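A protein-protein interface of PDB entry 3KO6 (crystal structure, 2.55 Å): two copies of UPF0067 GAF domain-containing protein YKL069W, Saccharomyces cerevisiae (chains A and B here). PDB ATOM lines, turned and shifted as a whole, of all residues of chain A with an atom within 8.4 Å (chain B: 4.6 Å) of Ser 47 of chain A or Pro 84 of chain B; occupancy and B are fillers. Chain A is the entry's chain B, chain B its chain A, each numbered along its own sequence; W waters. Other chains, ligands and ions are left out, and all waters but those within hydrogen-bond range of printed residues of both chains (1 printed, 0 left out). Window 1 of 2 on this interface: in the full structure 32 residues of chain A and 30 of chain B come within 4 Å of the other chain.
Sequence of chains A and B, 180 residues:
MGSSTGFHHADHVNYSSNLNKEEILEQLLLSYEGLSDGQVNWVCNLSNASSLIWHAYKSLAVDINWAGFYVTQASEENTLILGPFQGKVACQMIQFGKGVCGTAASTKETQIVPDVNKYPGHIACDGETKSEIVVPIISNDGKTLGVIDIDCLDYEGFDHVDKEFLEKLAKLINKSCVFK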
ATOM      1  N   TYR A  32      10.416  36.002   4.616  1.00  0.00           N
ATOM      2  CA  TYR A  32      10.487  34.665   4.014  1.00  0.00           C
ATOM      3  C   TYR A  32      11.345  34.676   2.742  1.00  0.00           C
ATOM      4  O   TYR A  32      12.244  33.842   2.569  1.00  0.00           O
ATOM      5  CB  TYR A  32       9.100  34.076   3.695  1.00  0.00           C
ATOM      6  CG  TYR A  32       9.291  32.782   2.964  1.00  0.00           C
ATOM      7  CD1 TYR A  32       9.545  31.603   3.662  1.00  0.00           C
ATOM      8  CD2 TYR A  32       9.337  32.747   1.575  1.00  0.00           C
ATOM      9  CE1 TYR A  32       9.798  30.409   2.993  1.00  0.00           C
ATOM     10  CE2 TYR A  32       9.586  31.556   0.902  1.00  0.00           C
ATOM     11  CZ  TYR A  32       9.822  30.390   1.624  1.00  0.00           C
ATOM     12  OH  TYR A  32      10.083  29.207   0.958  1.00  0.00           O
ATOM     13  N   LEU A  35      14.945  35.116   3.483  1.00  0.00           N
ATOM     14  CA  LEU A  35      15.486  33.963   4.188  1.00  0.00           C
ATOM     15  C   LEU A  35      15.580  32.723   3.314  1.00  0.00           C
ATOM     16  O   LEU A  35      16.465  31.898   3.513  1.00  0.00           O
ATOM     17  CB  LEU A  35      14.655  33.658   5.438  1.00  0.00           C
ATOM     18  CG  LEU A  35      14.661  34.731   6.532  1.00  0.00           C
ATOM     19  CD1 LEU A  35      13.466  34.524   7.469  1.00  0.00           C
ATOM     20  CD2 LEU A  35      16.006  34.777   7.288  1.00  0.00           C
ATOM     21  N   ASN A  41      16.423  24.234  -0.213  1.00  0.00           N
ATOM     22  CA  ASN A  41      16.151  23.223   0.824  1.00  0.00           C
ATOM     23  C   ASN A  41      14.832  23.482   1.559  1.00  0.00           C
ATOM     24  O   ASN A  41      14.679  24.497   2.255  1.00  0.00           O
ATOM     25  CB  ASN A  41      17.311  23.158   1.832  1.00  0.00           C
ATOM     26  CG  ASN A  41      17.197  21.970   2.786  1.00  0.00           C
ATOM     27  OD1 ASN A  41      16.361  21.956   3.713  1.00  0.00           O
ATOM     28  ND2 ASN A  41      18.040  20.962   2.563  1.00  0.00           N
ATOM     29  N   TRP A  42      13.876  22.574   1.408  1.00  0.00           N
ATOM     30  CA  TRP A  42      12.541  22.865   1.911  1.00  0.00           C
ATOM     31  C   TRP A  42      12.427  22.798   3.437  1.00  0.00           C
ATOM     32  O   TRP A  42      11.582  23.486   4.019  1.00  0.00           O
ATOM     33  CB  TRP A  42      11.458  22.043   1.203  1.00  0.00           C
ATOM     34  CG  TRP A  42      11.447  20.549   1.516  1.00  0.00           C
ATOM     35  CD1 TRP A  42      11.995  19.548   0.761  1.00  0.00           C
ATOM     36  CD2 TRP A  42      10.829  19.903   2.643  1.00  0.00           C
ATOM     37  NE1 TRP A  42      11.768  18.321   1.354  1.00  0.00           N
ATOM     38  CE2 TRP A  42      11.058  18.510   2.507  1.00  0.00           C
ATOM     39  CE3 TRP A  42      10.115  20.369   3.765  1.00  0.00           C
ATOM     40  CZ2 TRP A  42      10.598  17.578   3.441  1.00  0.00           C
ATOM     41  CZ3 TRP A  42       9.661  19.439   4.703  1.00  0.00           C
ATOM     42  CH2 TRP A  42       9.905  18.055   4.527  1.00  0.00           C
ATOM     43  N   VAL A  43      13.277  22.003   4.091  1.00  0.00           N
ATOM     44  CA  VAL A  43      13.179  21.871   5.546  1.00  0.00           C
ATOM     45  C   VAL A  43      13.670  23.156   6.166  1.00  0.00           C
ATOM     46  O   VAL A  43      13.024  23.709   7.057  1.00  0.00           O
ATOM     47  CB  VAL A  43      13.954  20.662   6.129  1.00  0.00           C
ATOM     48  CG1 VAL A  43      13.825  20.633   7.642  1.00  0.00           C
ATOM     49  CG2 VAL A  43      13.451  19.335   5.545  1.00  0.00           C
ATOM     50  N   CYS A  44      14.797  23.647   5.663  1.00  0.00           N
ATOM     51  CA  CYS A  44      15.369  24.904   6.110  1.00  0.00           C
ATOM     52  C   CYS A  44      14.372  26.036   5.892  1.00  0.00           C
ATOM     53  O   CYS A  44      14.062  26.803   6.806  1.00  0.00           O
ATOM     54  CB  CYS A  44      16.680  25.144   5.360  1.00  0.00           C
ATOM     55  SG  CYS A  44      17.289  26.831   5.327  1.00  0.00           S
ATOM     56  N   ASN A  45      13.833  26.107   4.685  1.00  0.00           N
ATOM     57  CA  ASN A  45      12.888  27.151   4.356  1.00  0.00           C
ATOM     58  C   ASN A  45      11.579  27.044   5.131  1.00  0.00           C
ATOM     59  O   ASN A  45      11.038  28.073   5.546  1.00  0.00           O
ATOM     60  CB  ASN A  45      12.657  27.202   2.846  1.00  0.00           C
ATOM     61  CG  ASN A  45      13.897  27.646   2.087  1.00  0.00           C
ATOM     62  OD1 ASN A  45      14.795  28.257   2.670  1.00  0.00           O
ATOM     63  ND2 ASN A  45      13.957  27.339   0.790  1.00  0.00           N
ATOM     64  N   LEU A  46      11.062  25.832   5.349  1.00  0.00           N
ATOM     65  CA  LEU A  46       9.805  25.718   6.118  1.00  0.00           C
ATOM     66  C   LEU A  46      10.005  25.836   7.632  1.00  0.00           C
ATOM     67  O   LEU A  46       9.090  26.229   8.353  1.00  0.00           O
ATOM     68  CB  LEU A  46       9.012  24.443   5.782  1.00  0.00           C
ATOM     69  CG  LEU A  46       8.499  24.223   4.348  1.00  0.00           C
ATOM     70  CD1 LEU A  46       7.400  23.193   4.346  1.00  0.00           C
ATOM     71  CD2 LEU A  46       8.043  25.504   3.665  1.00  0.00           C
ATOM     72  N   SER A  47      11.191  25.491   8.120  1.00  0.00           N
ATOM     73  CA  SER A  47      11.491  25.706   9.516  1.00  0.00           C
ATOM     74  C   SER A  47      11.383  27.185   9.865  1.00  0.00           C
ATOM     75  O   SER A  47      10.499  27.559  10.651  1.00  0.00           O
ATOM     76  CB  SER A  47      12.848  25.133   9.869  1.00  0.00           C
ATOM     77  OG  SER A  47      12.789  23.716   9.757  1.00  0.00           O
ATOM     78  N   ASN A  48      12.235  28.025   9.264  1.00  0.00           N
ATOM     79  CA  ASN A  48      12.133  29.486   9.429  1.00  0.00           C
ATOM     80  C   ASN A  48      10.726  30.021   9.192  1.00  0.00           C
ATOM     81  O   ASN A  48      10.263  30.882   9.935  1.00  0.00           O
ATOM     82  CB  ASN A  48      13.139  30.241   8.549  1.00  0.00           C
ATOM     83  CG  ASN A  48      14.565  30.173   9.097  1.00  0.00           C
ATOM     84  OD1 ASN A  48      14.769  30.086  10.308  1.00  0.00           O
ATOM     85  ND2 ASN A  48      15.552  30.204   8.206  1.00  0.00           N
ATOM     86  N   ALA A  49      10.018  29.502   8.194  1.00  0.00           N
ATOM     87  CA  ALA A  49       8.640  29.975   7.949  1.00  0.00           C
ATOM     88  C   ALA A  49       7.713  29.693   9.129  1.00  0.00           C
ATOM     89  O   ALA A  49       6.824  30.521   9.428  1.00  0.00           O
ATOM     90  CB  ALA A  49       8.063  29.385   6.674  1.00  0.00           C
ATOM     91  N   SER A  50       7.894  28.551   9.802  1.00  0.00           N
ATOM     92  CA  SER A  50       7.059  28.273  10.976  1.00  0.00           C
ATOM     93  C   SER A  50       7.311  29.316  12.066  1.00  0.00           C
ATOM     94  O   SER A  50       6.371  29.819  12.693  1.00  0.00           O
ATOM     95  CB  SER A  50       7.212  26.826  11.488  1.00  0.00           C
ATOM     96  OG  SER A  50       8.496  26.562  12.029  1.00  0.00           O
ATOM     97  N   SER A  51       8.574  29.698  12.236  1.00  0.00           N
ATOM     98  CA  SER A  51       8.922  30.738  13.182  1.00  0.00           C
ATOM     99  C   SER A  51       8.331  32.096  12.804  1.00  0.00           C
ATOM    100  O   SER A  51       7.815  32.823  13.667  1.00  0.00           O
ATOM    101  CB  SER A  51      10.422  30.846  13.320  1.00  0.00           C
ATOM    102  OG  SER A  51      10.710  31.701  14.408  1.00  0.00           O
ATOM    103  N   LEU A  52       8.391  32.433  11.516  1.00  0.00           N
ATOM    104  CA  LEU A  52       7.808  33.688  11.049  1.00  0.00           C
ATOM    105  C   LEU A  52       6.328  33.722  11.338  1.00  0.00           C
ATOM    106  O   LEU A  52       5.833  34.706  11.901  1.00  0.00           O
ATOM    107  CB  LEU A  52       8.056  33.919   9.553  1.00  0.00           C
ATOM    108  CG  LEU A  52       9.485  34.273   9.131  1.00  0.00           C
ATOM    109  CD1 LEU A  52       9.580  34.258   7.609  1.00  0.00           C
ATOM    110  CD2 LEU A  52       9.922  35.622   9.705  1.00  0.00           C
ATOM    111  N   ILE A  53       5.622  32.656  10.959  1.00  0.00           N
ATOM    112  CA  ILE A  53       4.180  32.592  11.152  1.00  0.00           C
ATOM    113  C   ILE A  53       3.872  32.670  12.643  1.00  0.00           C
ATOM    114  O   ILE A  53       3.095  33.531  13.060  1.00  0.00           O
ATOM    115  CB  ILE A  53       3.596  31.315  10.523  1.00  0.00           C
ATOM    116  CG1 ILE A  53       3.863  31.319   9.012  1.00  0.00           C
ATOM    117  CG2 ILE A  53       2.113  31.150  10.851  1.00  0.00           C
ATOM    118  CD1 ILE A  53       3.384  30.106   8.320  1.00  0.00           C
ATOM    119  N   TRP A  54       4.513  31.810  13.444  1.00  0.00           N
ATOM    120  CA  TRP A  54       4.260  31.767  14.894  1.00  0.00           C
ATOM    121  C   TRP A  54       4.296  33.161  15.503  1.00  0.00           C
ATOM    122  O   TRP A  54       3.298  33.618  16.060  1.00  0.00           O
ATOM    123  CB  TRP A  54       5.243  30.837  15.630  1.00  0.00           C
ATOM    124  CG  TRP A  54       5.065  30.849  17.154  1.00  0.00           C
ATOM    125  CD1 TRP A  54       5.649  31.711  18.034  1.00  0.00           C
ATOM    126  CD2 TRP A  54       4.260  29.959  17.947  1.00  0.00           C
ATOM    127  NE1 TRP A  54       5.255  31.427  19.315  1.00  0.00           N
ATOM    128  CE2 TRP A  54       4.402  30.358  19.296  1.00  0.00           C
ATOM    129  CE3 TRP A  54       3.425  28.872  17.648  1.00  0.00           C
ATOM    130  CZ2 TRP A  54       3.732  29.714  20.353  1.00  0.00           C
ATOM    131  CZ3 TRP A  54       2.752  28.236  18.699  1.00  0.00           C
ATOM    132  CH2 TRP A  54       2.916  28.663  20.037  1.00  0.00           C
ATOM    133  N   ALA A  67       1.792  26.413  14.656  1.00  0.00           N
ATOM    134  CA  ALA A  67       2.011  27.026  13.329  1.00  0.00           C
ATOM    135  C   ALA A  67       3.057  26.238  12.574  1.00  0.00           C
ATOM    136  O   ALA A  67       4.203  26.140  13.010  1.00  0.00           O
ATOM    137  CB  ALA A  67       2.462  28.489  13.468  1.00  0.00           C
ATOM    138  N   GLY A  68       2.683  25.641  11.458  1.00  0.00           N
ATOM    139  CA  GLY A  68       3.641  24.746  10.827  1.00  0.00           C
ATOM    140  C   GLY A  68       3.142  24.153   9.550  1.00  0.00           C
ATOM    141  O   GLY A  68       2.203  24.688   8.958  1.00  0.00           O
ATOM    142  N   PHE A  69       3.766  23.042   9.150  1.00  0.00           N
ATOM    143  CA  PHE A  69       3.557  22.434   7.830  1.00  0.00           C
ATOM    144  C   PHE A  69       3.352  20.913   7.863  1.00  0.00           C
ATOM    145  O   PHE A  69       3.842  20.221   8.769  1.00  0.00           O
ATOM    146  CB  PHE A  69       4.750  22.770   6.934  1.00  0.00           C
ATOM    147  CG  PHE A  69       4.929  24.241   6.708  1.00  0.00           C
ATOM    148  CD1 PHE A  69       5.727  25.002   7.564  1.00  0.00           C
ATOM    149  CD2 PHE A  69       4.277  24.872   5.658  1.00  0.00           C
ATOM    150  CE1 PHE A  69       5.874  26.369   7.384  1.00  0.00           C
ATOM    151  CE2 PHE A  69       4.410  26.243   5.455  1.00  0.00           C
ATOM    152  CZ  PHE A  69       5.208  27.003   6.322  1.00  0.00           C
ATOM    153  N   LEU A  82       4.089  14.926   8.776  1.00  0.00           N
ATOM    154  CA  LEU A  82       4.442  16.071   9.619  1.00  0.00           C
ATOM    155  C   LEU A  82       5.744  16.740   9.205  1.00  0.00           C
ATOM    156  O   LEU A  82       6.772  16.071   9.067  1.00  0.00           O
ATOM    157  CB  LEU A  82       4.524  15.654  11.092  1.00  0.00           C
ATOM    158  CG  LEU A  82       4.985  16.717  12.106  1.00  0.00           C
ATOM    159  CD1 LEU A  82       3.996  17.834  12.214  1.00  0.00           C
ATOM    160  CD2 LEU A  82       5.175  16.072  13.465  1.00  0.00           C
ATOM    161  N   GLY A  83       5.674  18.062   9.015  1.00  0.00           N
ATOM    162  CA  GLY A  83       6.830  18.879   8.678  1.00  0.00           C
ATOM    163  C   GLY A  83       7.154  19.830   9.809  1.00  0.00           C
ATOM    164  O   GLY A  83       6.616  19.682  10.908  1.00  0.00           O
ATOM    165  N   PRO A  84       8.048  20.814   9.562  1.00  0.00           N
ATOM    166  CA  PRO A  84       8.469  21.733  10.621  1.00  0.00           C
ATOM    167  C   PRO A  84       7.305  22.526  11.184  1.00  0.00           C
ATOM    168  O   PRO A  84       6.396  22.910  10.426  1.00  0.00           O
ATOM    169  CB  PRO A  84       9.448  22.684   9.910  1.00  0.00           C
ATOM    170  CG  PRO A  84       9.958  21.921   8.740  1.00  0.00           C
ATOM    171  CD  PRO A  84       8.793  21.037   8.306  1.00  0.00           C
ATOM    172  N   PHE A  85       7.344  22.771  12.497  1.00  0.00           N
ATOM    173  CA  PHE A  85       6.327  23.569  13.160  1.00  0.00           C
ATOM    174  C   PHE A  85       6.855  24.213  14.415  1.00  0.00           C
ATOM    175  O   PHE A  85       7.858  23.766  14.981  1.00  0.00           O
ATOM    176  CB  PHE A  85       5.129  22.716  13.552  1.00  0.00           C
ATOM    177  CG  PHE A  85       5.441  21.638  14.573  1.00  0.00           C
ATOM    178  CD1 PHE A  85       5.246  21.868  15.933  1.00  0.00           C
ATOM    179  CD2 PHE A  85       5.907  20.378  14.164  1.00  0.00           C
ATOM    180  CE1 PHE A  85       5.518  20.865  16.876  1.00  0.00           C
ATOM    181  CE2 PHE A  85       6.189  19.376  15.104  1.00  0.00           C
ATOM    182  CZ  PHE A  85       5.996  19.619  16.449  1.00  0.00           C
ATOM    183  N   GLN A  86       6.167  25.274  14.833  1.00  0.00           N
ATOM    184  CA  GLN A  86       6.264  25.788  16.195  1.00  0.00           C
ATOM    185  C   GLN A  86       4.970  25.372  16.853  1.00  0.00           C
ATOM    186  O   GLN A  86       3.878  25.524  16.254  1.00  0.00           O
ATOM    187  CB  GLN A  86       6.337  27.319  16.209  1.00  0.00           C
ATOM    188  CG  GLN A  86       7.393  27.924  15.297  1.00  0.00           C
ATOM    189  CD  GLN A  86       8.765  27.740  15.850  1.00  0.00           C
ATOM    190  OE1 GLN A  86       9.035  28.089  17.009  1.00  0.00           O
ATOM    191  NE2 GLN A  86       9.654  27.160  15.041  1.00  0.00           N
ATOM    192  N   CYS A 177      11.282  26.570  -2.996  1.00  0.00           N
ATOM    193  CA  CYS A 177      11.640  25.261  -2.440  1.00  0.00           C
ATOM    194  C   CYS A 177      11.541  24.158  -3.484  1.00  0.00           C
ATOM    195  O   CYS A 177      10.647  24.171  -4.339  1.00  0.00           O
ATOM    196  CB  CYS A 177      10.721  24.881  -1.271  1.00  0.00           C
ATOM    197  SG  CYS A 177      10.711  25.992   0.126  1.00  0.00           S
ATOM    198  N   TRP B  42      12.716  11.507   8.922  1.00  0.00           N
ATOM    199  CA  TRP B  42      13.503  12.298   9.853  1.00  0.00           C
ATOM    200  C   TRP B  42      12.932  13.706  10.131  1.00  0.00           C
ATOM    201  O   TRP B  42      13.104  14.239  11.235  1.00  0.00           O
ATOM    202  CB  TRP B  42      14.976  12.329   9.430  1.00  0.00           C
ATOM    203  CG  TRP B  42      15.291  13.160   8.239  1.00  0.00           C
ATOM    204  CD1 TRP B  42      15.428  12.733   6.940  1.00  0.00           C
ATOM    205  CD2 TRP B  42      15.548  14.558   8.227  1.00  0.00           C
ATOM    206  NE1 TRP B  42      15.751  13.786   6.116  1.00  0.00           N
ATOM    207  CE2 TRP B  42      15.836  14.923   6.878  1.00  0.00           C
ATOM    208  CE3 TRP B  42      15.555  15.551   9.216  1.00  0.00           C
ATOM    209  CZ2 TRP B  42      16.126  16.240   6.501  1.00  0.00           C
ATOM    210  CZ3 TRP B  42      15.851  16.863   8.844  1.00  0.00           C
ATOM    211  CH2 TRP B  42      16.130  17.194   7.495  1.00  0.00           C
ATOM    212  N   VAL B  43      12.241  14.285   9.145  1.00  0.00           N
ATOM    213  CA  VAL B  43      11.658  15.620   9.293  1.00  0.00           C
ATOM    214  C   VAL B  43      10.571  15.585  10.360  1.00  0.00           C
ATOM    215  O   VAL B  43      10.515  16.469  11.224  1.00  0.00           O
ATOM    216  CB  VAL B  43      11.105  16.176   7.960  1.00  0.00           C
ATOM    217  CG1 VAL B  43      10.556  17.586   8.152  1.00  0.00           C
ATOM    218  CG2 VAL B  43      12.184  16.177   6.890  1.00  0.00           C
ATOM    219  N   LEU B  46      12.246  14.723  14.037  1.00  0.00           N
ATOM    220  CA  LEU B  46      12.988  15.842  14.623  1.00  0.00           C
ATOM    221  C   LEU B  46      12.080  17.020  14.947  1.00  0.00           C
ATOM    222  O   LEU B  46      12.263  17.658  15.988  1.00  0.00           O
ATOM    223  CB  LEU B  46      14.174  16.287  13.762  1.00  0.00           C
ATOM    224  CG  LEU B  46      15.285  15.280  13.416  1.00  0.00           C
ATOM    225  CD1 LEU B  46      16.561  16.012  13.048  1.00  0.00           C
ATOM    226  CD2 LEU B  46      15.565  14.269  14.519  1.00  0.00           C
ATOM    227  N   SER B  47      11.110  17.312  14.076  1.00  0.00           N
ATOM    228  CA  SER B  47      10.125  18.357  14.358  1.00  0.00           C
ATOM    229  C   SER B  47       9.518  18.122  15.721  1.00  0.00           C
ATOM    230  O   SER B  47       9.638  18.970  16.610  1.00  0.00           O
ATOM    231  CB  SER B  47       9.045  18.403  13.287  1.00  0.00           C
ATOM    232  OG  SER B  47       9.582  18.934  12.086  1.00  0.00           O
ATOM    233  N   SER B  50      11.940  18.473  18.596  1.00  0.00           N
ATOM    234  CA  SER B  50      12.243  19.855  18.924  1.00  0.00           C
ATOM    235  C   SER B  50      11.219  20.389  19.910  1.00  0.00           C
ATOM    236  O   SER B  50      11.574  21.077  20.868  1.00  0.00           O
ATOM    237  CB  SER B  50      12.358  20.741  17.655  1.00  0.00           C
ATOM    238  OG  SER B  50      11.106  21.224  17.163  1.00  0.00           O
ATOM    239  N   GLY B  68      16.503  22.848  18.594  1.00  0.00           N
ATOM    240  CA  GLY B  68      16.313  22.233  17.278  1.00  0.00           C
ATOM    241  C   GLY B  68      17.540  21.539  16.695  1.00  0.00           C
ATOM    242  O   GLY B  68      18.453  21.142  17.427  1.00  0.00           O
ATOM    243  N   PHE B  69      17.569  21.407  15.368  1.00  0.00           N
ATOM    244  CA  PHE B  69      18.582  20.593  14.691  1.00  0.00           C
ATOM    245  C   PHE B  69      19.166  21.220  13.431  1.00  0.00           C
ATOM    246  O   PHE B  69      18.514  22.026  12.735  1.00  0.00           O
ATOM    247  CB  PHE B  69      17.974  19.247  14.288  1.00  0.00           C
ATOM    248  CG  PHE B  69      17.329  18.512  15.421  1.00  0.00           C
ATOM    249  CD1 PHE B  69      16.002  18.777  15.777  1.00  0.00           C
ATOM    250  CD2 PHE B  69      18.045  17.557  16.141  1.00  0.00           C
ATOM    251  CE1 PHE B  69      15.396  18.105  16.833  1.00  0.00           C
ATOM    252  CE2 PHE B  69      17.446  16.869  17.204  1.00  0.00           C
ATOM    253  CZ  PHE B  69      16.123  17.138  17.543  1.00  0.00           C
ATOM    254  N   LEU B  82      19.930  23.938   8.020  1.00  0.00           N
ATOM    255  CA  LEU B  82      18.913  24.131   9.061  1.00  0.00           C
ATOM    256  C   LEU B  82      17.786  23.108   8.995  1.00  0.00           C
ATOM    257  O   LEU B  82      17.218  22.888   7.930  1.00  0.00           O
ATOM    258  CB  LEU B  82      18.323  25.542   9.004  1.00  0.00           C
ATOM    259  CG  LEU B  82      17.272  25.918  10.058  1.00  0.00           C
ATOM    260  CD1 LEU B  82      17.870  25.941  11.457  1.00  0.00           C
ATOM    261  CD2 LEU B  82      16.604  27.250   9.738  1.00  0.00           C
ATOM    262  N   GLY B  83      17.486  22.485  10.137  1.00  0.00           N
ATOM    263  CA  GLY B  83      16.364  21.564  10.236  1.00  0.00           C
ATOM    264  C   GLY B  83      15.291  22.108  11.167  1.00  0.00           C
ATOM    265  O   GLY B  83      15.326  23.278  11.541  1.00  0.00           O
ATOM    266  N   PRO B  84      14.338  21.250  11.569  1.00  0.00           N
ATOM    267  CA  PRO B  84      13.238  21.647  12.438  1.00  0.00           C
ATOM    268  C   PRO B  84      13.729  22.268  13.736  1.00  0.00           C
ATOM    269  O   PRO B  84      14.824  21.921  14.229  1.00  0.00           O
ATOM    270  CB  PRO B  84      12.542  20.319  12.737  1.00  0.00           C
ATOM    271  CG  PRO B  84      12.848  19.475  11.572  1.00  0.00           C
ATOM    272  CD  PRO B  84      14.279  19.813  11.252  1.00  0.00           C
ATOM    273  N   PHE B  85      12.937  23.179  14.296  1.00  0.00           N
ATOM    274  CA  PHE B  85      13.343  23.809  15.535  1.00  0.00           C
ATOM    275  C   PHE B  85      12.213  24.540  16.170  1.00  0.00           C
ATOM    276  O   PHE B  85      11.263  24.930  15.488  1.00  0.00           O
ATOM    277  CB  PHE B  85      14.500  24.788  15.292  1.00  0.00           C
ATOM    278  CG  PHE B  85      14.117  26.034  14.510  1.00  0.00           C
ATOM    279  CD1 PHE B  85      13.624  27.159  15.156  1.00  0.00           C
ATOM    280  CD2 PHE B  85      14.290  26.088  13.129  1.00  0.00           C
ATOM    281  CE1 PHE B  85      13.295  28.315  14.434  1.00  0.00           C
ATOM    282  CE2 PHE B  85      13.960  27.242  12.410  1.00  0.00           C
ATOM    283  CZ  PHE B  85      13.471  28.350  13.064  1.00  0.00           C
HETATM  284  O   HOH W   1      17.394  20.622   6.483  1.00  0.00           O
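Of the printed residues of chain B, Val 43 of chain A touches Trp 42, Val 43, Leu 82, Gly 83 and Pro 84. Of chain B, only Gly 83, Pro 84 and Phe 85 come within 4 Å of Ser 47 of chain A. Ser 50 of chain B touches none of the printed residues of chain A. Gly 68 of chain B touches none of the printed residues of chain A. Of the printed residues of chain A, Leu 82 of chain B touches Val 43 (3.97 Å), Cys 44 (3.3 Å) and Asn 48 (3.4 Å). Of the printed residues of chain A, Gly 83 of chain B touches Val 43 (3.7 Å) and Ser 47 (3.1 Å). Pro 84 of chain B touches just these residues of chain A: Val 43 (3.7 Å) and Ser 47 (3.4 Å). Printed residues of chain A within 4 Å of Phe 85 of chain B: Ser 47 (3.5 Å), Asn 48 (3.5 Å), Ser 51 (3.9 Å), Phe 85 (3.6 Å) and Gln 86 (2.8 Å). The nearest residue of chain B that does not touch Ser 47 of chain A is Leu 82 of chain B (4.3 Å). The nearest printed residue of chain B that does not touch Pro 84 of chain A is Pro 84 of chain B (4.7 Å).
Hydrophobic or aromatic side chains of chain B that line the printed part of chain A: Trp 42, Val 43, Leu 82, Pro 84 and Phe 85. Along chain B the printed residues that touch a printed residue of chain A span positions 42 to 85. Printed residues of chain A that touch a printed residue of chain B: Trp 42, Val 43, Cys 44, Ser 47, Asn 48, Ser 51, Gly 83, Pro 84, Phe 85 and Gln 86. Hydrophobic or aromatic side chains of chain A that line the printed part of chain B: Trp 42, Val 43, Pro 84 and Phe 85. Among the printed residues, 20 pairs touch across the chains. Among the printed residues, no Asp or Glu carboxylate lies within 4 Å of a Lys or Arg side-chain nitrogen of the other chain.
Trp 42 of chain A touches Val 43 of chain B, and with the chains exchanged Val 43 of chain A touches Trp 42 of chain B. Val 43 of chain A touches Leu 82 of chain B, but with the chains exchanged Leu 82 of chain A does not touch Val 43 of chain B (4.04 Å). Ser 47 of chain A touches Phe 85 of chain B, and with the chains exchanged Phe 85 of chain A touches Ser 47 of chain B. Phe 85 of chain B touches its own counterpart, Phe 85 of chain A. Of the 20 pairs that touch across the chains among the printed residues, 14 have their exchanged pair printed and touching as well.
Val 43 of chain B touches Trp 42 of chain A. CH2 of Trp 42 of chain B touches CG2 of Val 43 of chain A, 3.9 Å away. O of Leu 82 of chain B touches C of Val 43 of chain A (3.97 Å). CA of Gly 83 of chain B touches CG1 of Val 43 of chain A (3.7 Å). Val 43 of chain A touches Pro 84 of chain B (CG1 to CD, 3.7 Å). Asn 48 of chain A touches Phe 85 of chain B (OD1 to CZ, 3.5 Å). Ser 51 of chain A touches Phe 85 of chain B. Gly 83 of chain A touches Val 43 of chain B. Pro 84 of chain A touches Val 43 of chain B. O of Phe 85 of chain A touches O of Phe 85 of chain B (3.6 Å).
Water W1 bridges the backbone carbonyl oxygen of Leu 82 of chain B and the side-chain amide oxygen of Asn 41 of chain A.
O of Val 43 of chain B is in hydrogen-bond range of OG of Ser 47 of chain B (2.8 Å). O of Phe 69 of chain A is in hydrogen-bond range of N of Gly 83 of chain A, 2.8 Å away. N of Ala 67 of chain A lies within hydrogen-bond range of O of Gln 86 of chain A. The side-chain amide oxygen (OD1) of Asn 41 of chain A is in hydrogen-bond range of the backbone NH (N) of Cys 44 of chain A (3.0 Å). The backbone carbonyl oxygen (O) of Ser 47 of chain A lies within hydrogen-bond range of the side-chain hydroxyl (OG) of Ser 50 of chain A. The backbone NH (N) of Gly 83 of chain B lies within hydrogen-bond range of the backbone carbonyl oxygen (O) of Phe 69 of chain B.
O of Leu 82 of chain B lies close to N of Cys 44 of chain A, 3.4 Å away. N of Pro 84 of chain B sits close to OG of Ser 47 of chain A. OG of Ser 47 of chain A lies within hydrogen-bond range of O of Gly 83 of chain B (3.1 Å). The side-chain hydroxyl (OG) of Ser 47 of chain B lies within hydrogen-bond range of the backbone carbonyl oxygen (O) of Gly 83 of chain A (3.3 Å). The backbone carbonyl oxygen (O) of Phe 85 of chain B sits at hydrogen-bond distance from the side-chain amide nitrogen (NE2) of Gln 86 of chain A (2.8 Å).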
